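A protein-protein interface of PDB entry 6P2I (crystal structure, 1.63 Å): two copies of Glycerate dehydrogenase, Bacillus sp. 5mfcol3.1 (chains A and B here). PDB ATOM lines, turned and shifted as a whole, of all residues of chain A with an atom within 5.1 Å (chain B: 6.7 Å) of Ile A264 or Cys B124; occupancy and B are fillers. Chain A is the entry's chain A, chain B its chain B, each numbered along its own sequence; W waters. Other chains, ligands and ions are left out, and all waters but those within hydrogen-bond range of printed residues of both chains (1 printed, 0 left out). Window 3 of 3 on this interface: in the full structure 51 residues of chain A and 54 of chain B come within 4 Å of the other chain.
Printed residues of chain A that touch a printed residue of chain B: Tyr A258, Ile A264, Leu A266, Leu A271, Thr A272 and Pro A273. Hydrophobic or aromatic side chains of chain A that line the printed part of chain B: Tyr A258, Ile A264, Leu A271 and Pro A273. Hydrophobic or aromatic side chains of chain B that line the printed part of chain A: Ala B120. Among the printed residues, 14 pairs touch across the chains. Among the printed residues, no Asp or Glu carboxylate lies within 4 Å of a Lys or Arg side-chain nitrogen of the other chain.
Water W1 lies within hydrogen-bond range of the side-chain hydroxyl of Tyr A258, the backbone carbonyl oxygen of Thr A272 and the side-chain sulfur of Cys B124.
Cys B124 touches four residues of chain A. Printed residues of chain A within 4 Å of Leu B128: Pro A273 (3.9 Å). Of the printed residues of chain B, Leu A266 touches Arg B125 (2.9 Å). Printed residues of chain B within 4 Å of Leu A271: Ala B120 (3.5 Å), Asp B121 (2.9 Å), Cys B124 (3.5 Å) and Arg B125 (3.96 Å). Printed residues of chain A within 4 Å of Ala B120: Leu A271 (3.5 Å), Thr A272 (3.9 Å) and Pro A273 (3.6 Å). Printed residues of chain A within 4 Å of Ser B129: Tyr A258 (3.5 Å). The nearest residue of chain A that does not touch Cys B124 is Tyr A258 (4.03 Å).
The guanidinium group (NH1) of Arg B125 is in hydrogen-bond range of the backbone carbonyl oxygen (O) of Ile A264 (2.9 Å). The backbone carbonyl oxygen (O) of Leu A266 sits at hydrogen-bond distance from the guanidinium group (NH1) of Arg B125, 2.9 Å away. O of Thr A272 lies close to SG of Cys B124, 3.6 Å away. SG of Cys B124 sits close to N of Pro A273. N of Leu A271 is in hydrogen-bond range of OD1 of Asp B121.
Among the printed residues, merely in contact across the chains: Tyr A258 with Gly B127 (3.5 Å), Tyr A258 with Ser B129 (3.5 Å), Leu A271 with Cys B124 (3.5 Å), Leu A271 with Ala B120 (3.5 Å), Pro A273 with Ala B120 (3.6 Å), Ile A264 with Cys B124 (3.7 Å), Pro A273 with Leu B128 (3.9 Å), Thr A272 with Ala B120 (3.9 Å) and Leu A271 with Arg B125 (3.96 Å).
The backbone NH of Leu A255 lies within hydrogen-bond range of the side-chain hydroxyl of Tyr A258 (3.2 Å). SG of Cys B124 lies within hydrogen-bond range of O of Ala B120, at 3.5 Å. The backbone carbonyl oxygen (O) of Thr B123 is in hydrogen-bond range of the backbone NH (N) of Leu B128 (3.3 Å). OD2 of Asp B121 is in salt-bridge range of NE of Arg B125.
No position is printed for both chains.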
ATOM      1  N   LEU A 255      29.436  32.474  20.619  1.00  0.00           N
ATOM      2  CA  LEU A 255      30.161  31.989  19.452  1.00  0.00           C
ATOM      3  C   LEU A 255      30.457  33.187  18.568  1.00  0.00           C
ATOM      4  O   LEU A 255      29.775  34.211  18.650  1.00  0.00           O
ATOM      5  CB  LEU A 255      29.366  30.956  18.643  1.00  0.00           C
ATOM      6  CG  LEU A 255      28.861  29.701  19.348  1.00  0.00           C
ATOM      7  CD1 LEU A 255      28.014  28.945  18.352  1.00  0.00           C
ATOM      8  CD2 LEU A 255      30.016  28.857  19.815  1.00  0.00           C
ATOM      9  N   TYR A 258      26.508  32.400  14.680  1.00  0.00           N
ATOM     10  CA  TYR A 258      25.594  31.309  14.993  1.00  0.00           C
ATOM     11  C   TYR A 258      25.030  30.630  13.750  1.00  0.00           C
ATOM     12  O   TYR A 258      25.171  29.415  13.611  1.00  0.00           O
ATOM     13  CB  TYR A 258      24.462  31.813  15.898  1.00  0.00           C
ATOM     14  CG  TYR A 258      24.927  31.982  17.321  1.00  0.00           C
ATOM     15  CD1 TYR A 258      25.642  33.111  17.698  1.00  0.00           C
ATOM     16  CD2 TYR A 258      24.674  31.004  18.281  1.00  0.00           C
ATOM     17  CE1 TYR A 258      26.089  33.275  18.983  1.00  0.00           C
ATOM     18  CE2 TYR A 258      25.122  31.154  19.582  1.00  0.00           C
ATOM     19  CZ  TYR A 258      25.826  32.293  19.927  1.00  0.00           C
ATOM     20  OH  TYR A 258      26.276  32.457  21.215  1.00  0.00           O
ATOM     21  N   ASN A 261      26.929  27.836  11.810  1.00  0.00           N
ATOM     22  CA  ASN A 261      28.181  27.523  12.488  1.00  0.00           C
ATOM     23  C   ASN A 261      28.232  26.025  12.759  1.00  0.00           C
ATOM     24  O   ASN A 261      27.322  25.491  13.405  1.00  0.00           O
ATOM     25  CB  ASN A 261      28.312  28.309  13.789  1.00  0.00           C
ATOM     26  CG  ASN A 261      29.714  28.237  14.386  1.00  0.00           C
ATOM     27  OD1 ASN A 261      30.342  27.175  14.420  1.00  0.00           O
ATOM     28  ND2 ASN A 261      30.202  29.368  14.880  1.00  0.00           N
ATOM     29  N   PRO A 262      29.257  25.314  12.280  1.00  0.00           N
ATOM     30  CA  PRO A 262      29.300  23.854  12.467  1.00  0.00           C
ATOM     31  C   PRO A 262      29.272  23.416  13.923  1.00  0.00           C
ATOM     32  O   PRO A 262      28.876  22.275  14.201  1.00  0.00           O
ATOM     33  CB  PRO A 262      30.618  23.454  11.790  1.00  0.00           C
ATOM     34  CG  PRO A 262      30.906  24.567  10.826  1.00  0.00           C
ATOM     35  CD  PRO A 262      30.392  25.809  11.481  1.00  0.00           C
ATOM     36  N   ILE A 263      29.678  24.275  14.859  1.00  0.00           N
ATOM     37  CA  ILE A 263      29.624  23.898  16.271  1.00  0.00           C
ATOM     38  C   ILE A 263      28.193  23.590  16.698  1.00  0.00           C
ATOM     39  O   ILE A 263      27.969  22.757  17.589  1.00  0.00           O
ATOM     40  CB  ILE A 263      30.262  25.010  17.125  1.00  0.00           C
ATOM     41  CG1 ILE A 263      31.770  25.058  16.866  1.00  0.00           C
ATOM     42  CG2 ILE A 263      29.959  24.819  18.616  1.00  0.00           C
ATOM     43  CD1 ILE A 263      32.489  26.122  17.641  1.00  0.00           C
ATOM     44  N   ILE A 264      27.205  24.217  16.050  1.00  0.00           N
ATOM     45  CA  ILE A 264      25.797  23.949  16.351  1.00  0.00           C
ATOM     46  C   ILE A 264      25.425  22.491  16.089  1.00  0.00           C
ATOM     47  O   ILE A 264      24.439  21.993  16.648  1.00  0.00           O
ATOM     48  CB  ILE A 264      24.901  24.932  15.552  1.00  0.00           C
ATOM     49  CG1 ILE A 264      24.572  26.152  16.406  1.00  0.00           C
ATOM     50  CG2 ILE A 264      23.619  24.288  15.054  1.00  0.00           C
ATOM     51  CD1 ILE A 264      25.760  26.964  16.745  1.00  0.00           C
ATOM     52  N   GLY A 265      26.215  21.778  15.289  1.00  0.00           N
ATOM     53  CA  GLY A 265      25.984  20.383  14.989  1.00  0.00           C
ATOM     54  C   GLY A 265      26.560  19.393  15.981  1.00  0.00           C
ATOM     55  O   GLY A 265      26.298  18.189  15.866  1.00  0.00           O
ATOM     56  N   LEU A 266      27.328  19.860  16.958  1.00  0.00           N
ATOM     57  CA  LEU A 266      28.061  18.981  17.863  1.00  0.00           C
ATOM     58  C   LEU A 266      27.192  18.513  19.024  1.00  0.00           C
ATOM     59  O   LEU A 266      26.426  19.290  19.602  1.00  0.00           O
ATOM     60  CB  LEU A 266      29.288  19.693  18.425  1.00  0.00           C
ATOM     61  CG  LEU A 266      30.383  20.120  17.455  1.00  0.00           C
ATOM     62  CD1 LEU A 266      31.351  21.052  18.176  1.00  0.00           C
ATOM     63  CD2 LEU A 266      31.098  18.906  16.913  1.00  0.00           C
ATOM     64  N   LEU A 271      25.231  25.065  24.652  1.00  0.00           N
ATOM     65  CA  LEU A 271      25.243  26.455  24.212  1.00  0.00           C
ATOM     66  C   LEU A 271      24.204  27.262  24.971  1.00  0.00           C
ATOM     67  O   LEU A 271      23.077  26.801  25.167  1.00  0.00           O
ATOM     68  CB  LEU A 271      24.951  26.535  22.716  1.00  0.00           C
ATOM     69  CG  LEU A 271      25.875  25.690  21.852  1.00  0.00           C
ATOM     70  CD1 LEU A 271      25.392  25.698  20.414  1.00  0.00           C
ATOM     71  CD2 LEU A 271      27.307  26.213  21.955  1.00  0.00           C
ATOM     72  N   THR A 272      24.580  28.468  25.394  1.00  0.00           N
ATOM     73  CA  THR A 272      23.602  29.406  25.917  1.00  0.00           C
ATOM     74  C   THR A 272      23.713  30.731  25.165  1.00  0.00           C
ATOM     75  O   THR A 272      24.806  31.123  24.741  1.00  0.00           O
ATOM     76  CB  THR A 272      23.765  29.601  27.437  1.00  0.00           C
ATOM     77  OG1 THR A 272      25.126  29.918  27.773  1.00  0.00           O
ATOM     78  CG2 THR A 272      23.384  28.288  28.177  1.00  0.00           C
ATOM     79  N   PRO A 273      22.595  31.426  24.951  1.00  0.00           N
ATOM     80  CA  PRO A 273      22.605  32.609  24.052  1.00  0.00           C
ATOM     81  C   PRO A 273      23.010  33.901  24.754  1.00  0.00           C
ATOM     82  O   PRO A 273      22.264  34.890  24.780  1.00  0.00           O
ATOM     83  CB  PRO A 273      21.152  32.649  23.552  1.00  0.00           C
ATOM     84  CG  PRO A 273      20.352  32.158  24.757  1.00  0.00           C
ATOM     85  CD  PRO A 273      21.232  31.063  25.391  1.00  0.00           C
ATOM     86  N   GLN B 119      16.114  24.814  27.023  1.00  0.00           N
ATOM     87  CA  GLN B 119      15.599  25.818  26.097  1.00  0.00           C
ATOM     88  C   GLN B 119      16.692  26.758  25.615  1.00  0.00           C
ATOM     89  O   GLN B 119      16.618  27.263  24.480  1.00  0.00           O
ATOM     90  CB  GLN B 119      14.486  26.627  26.759  1.00  0.00           C
ATOM     91  CG  GLN B 119      13.175  25.883  26.945  1.00  0.00           C
ATOM     92  CD  GLN B 119      13.037  25.262  28.326  1.00  0.00           C
ATOM     93  OE1 GLN B 119      14.008  25.161  29.098  1.00  0.00           O
ATOM     94  NE2 GLN B 119      11.819  24.827  28.641  1.00  0.00           N
ATOM     95  N   ALA B 120      17.675  27.051  26.471  1.00  0.00           N
ATOM     96  CA  ALA B 120      18.744  27.958  26.064  1.00  0.00           C
ATOM     97  C   ALA B 120      19.577  27.340  24.961  1.00  0.00           C
ATOM     98  O   ALA B 120      19.921  28.013  23.980  1.00  0.00           O
ATOM     99  CB  ALA B 120      19.622  28.332  27.264  1.00  0.00           C
ATOM    100  N   ASP B 121      19.899  26.057  25.099  1.00  0.00           N
ATOM    101  CA  ASP B 121      20.660  25.383  24.062  1.00  0.00           C
ATOM    102  C   ASP B 121      19.868  25.314  22.766  1.00  0.00           C
ATOM    103  O   ASP B 121      20.408  25.570  21.685  1.00  0.00           O
ATOM    104  CB  ASP B 121      21.063  23.989  24.542  1.00  0.00           C
ATOM    105  CG  ASP B 121      21.888  23.260  23.525  1.00  0.00           C
ATOM    106  OD1 ASP B 121      23.129  23.356  23.604  1.00  0.00           O
ATOM    107  OD2 ASP B 121      21.290  22.616  22.632  1.00  0.00           O
ATOM    108  N   GLU B 122      18.575  25.001  22.860  1.00  0.00           N
ATOM    109  CA  GLU B 122      17.748  24.933  21.662  1.00  0.00           C
ATOM    110  C   GLU B 122      17.696  26.281  20.953  1.00  0.00           C
ATOM    111  O   GLU B 122      17.726  26.334  19.723  1.00  0.00           O
ATOM    112  CB  GLU B 122      16.348  24.450  22.032  1.00  0.00           C
ATOM    113  CG  GLU B 122      15.365  24.490  20.872  1.00  0.00           C
ATOM    114  CD  GLU B 122      13.951  24.108  21.280  1.00  0.00           C
ATOM    115  OE1 GLU B 122      13.512  24.499  22.382  1.00  0.00           O
ATOM    116  OE2 GLU B 122      13.276  23.417  20.489  1.00  0.00           O
ATOM    117  N   THR B 123      17.663  27.380  21.717  1.00  0.00           N
ATOM    118  CA  THR B 123      17.660  28.717  21.120  1.00  0.00           C
ATOM    119  C   THR B 123      18.898  28.927  20.259  1.00  0.00           C
ATOM    120  O   THR B 123      18.815  29.433  19.134  1.00  0.00           O
ATOM    121  CB  THR B 123      17.599  29.767  22.234  1.00  0.00           C
ATOM    122  OG1 THR B 123      16.382  29.613  22.972  1.00  0.00           O
ATOM    123  CG2 THR B 123      17.686  31.184  21.668  1.00  0.00           C
ATOM    124  N   CYS B 124      20.061  28.535  20.780  1.00  0.00           N
ATOM    125  CA  CYS B 124      21.305  28.682  20.032  1.00  0.00           C
ATOM    126  C   CYS B 124      21.332  27.783  18.804  1.00  0.00           C
ATOM    127  O   CYS B 124      21.849  28.184  17.756  1.00  0.00           O
ATOM    128  CB  CYS B 124      22.496  28.376  20.940  1.00  0.00           C
ATOM    129  SG  CYS B 124      22.664  29.507  22.333  1.00  0.00           S
ATOM    130  N   ARG B 125      20.805  26.557  18.912  1.00  0.00           N
ATOM    131  CA  ARG B 125      20.778  25.679  17.745  1.00  0.00           C
ATOM    132  C   ARG B 125      19.907  26.254  16.642  1.00  0.00           C
ATOM    133  O   ARG B 125      20.108  25.948  15.460  1.00  0.00           O
ATOM    134  CB  ARG B 125      20.267  24.281  18.107  1.00  0.00           C
ATOM    135  CG  ARG B 125      20.856  23.648  19.332  1.00  0.00           C
ATOM    136  CD  ARG B 125      22.264  23.151  19.116  1.00  0.00           C
ATOM    137  NE  ARG B 125      22.817  22.693  20.388  1.00  0.00           N
ATOM    138  CZ  ARG B 125      23.916  21.960  20.526  1.00  0.00           C
ATOM    139  NH1 ARG B 125      24.606  21.572  19.462  1.00  0.00           N
ATOM    140  NH2 ARG B 125      24.318  21.616  21.741  1.00  0.00           N
ATOM    141  N   LYS B 126      18.934  27.088  17.005  1.00  0.00           N
ATOM    142  CA  LYS B 126      18.143  27.796  16.011  1.00  0.00           C
ATOM    143  C   LYS B 126      18.852  29.029  15.473  1.00  0.00           C
ATOM    144  O   LYS B 126      18.267  29.754  14.662  1.00  0.00           O
ATOM    145  CB  LYS B 126      16.783  28.172  16.602  1.00  0.00           C
ATOM    146  CG  LYS B 126      15.974  26.964  17.052  1.00  0.00           C
ATOM    147  CD  LYS B 126      14.552  27.337  17.430  1.00  0.00           C
ATOM    148  CE  LYS B 126      14.515  28.241  18.649  1.00  0.00           C
ATOM    149  NZ  LYS B 126      13.181  28.881  18.810  1.00  0.00           N
ATOM    150  N   GLY B 127      20.086  29.282  15.901  1.00  0.00           N
ATOM    151  CA  GLY B 127      20.876  30.365  15.357  1.00  0.00           C
ATOM    152  C   GLY B 127      20.678  31.711  16.016  1.00  0.00           C
ATOM    153  O   GLY B 127      21.109  32.724  15.450  1.00  0.00           O
ATOM    154  N   LEU B 128      20.043  31.759  17.181  1.00  0.00           N
ATOM    155  CA  LEU B 128      19.720  33.010  17.853  1.00  0.00           C
ATOM    156  C   LEU B 128      20.743  33.309  18.943  1.00  0.00           C
ATOM    157  O   LEU B 128      21.158  32.415  19.691  1.00  0.00           O
ATOM    158  CB  LEU B 128      18.307  32.950  18.445  1.00  0.00           C
ATOM    159  CG  LEU B 128      17.176  32.702  17.433  1.00  0.00           C
ATOM    160  CD1 LEU B 128      15.853  32.646  18.165  1.00  0.00           C
ATOM    161  CD2 LEU B 128      17.125  33.785  16.342  1.00  0.00           C
ATOM    162  N   SER B 129      21.142  34.575  19.029  1.00  0.00           N
ATOM    163  CA  SER B 129      22.157  35.038  19.960  1.00  0.00           C
ATOM    164  C   SER B 129      21.591  36.154  20.836  1.00  0.00           C
ATOM    165  O   SER B 129      20.612  36.818  20.479  1.00  0.00           O
ATOM    166  CB  SER B 129      23.402  35.540  19.211  1.00  0.00           C
ATOM    167  OG  SER B 129      23.112  36.737  18.518  1.00  0.00           O
HETATM  168  O   HOH W   1      26.352  30.139  22.658  1.00  0.00           O
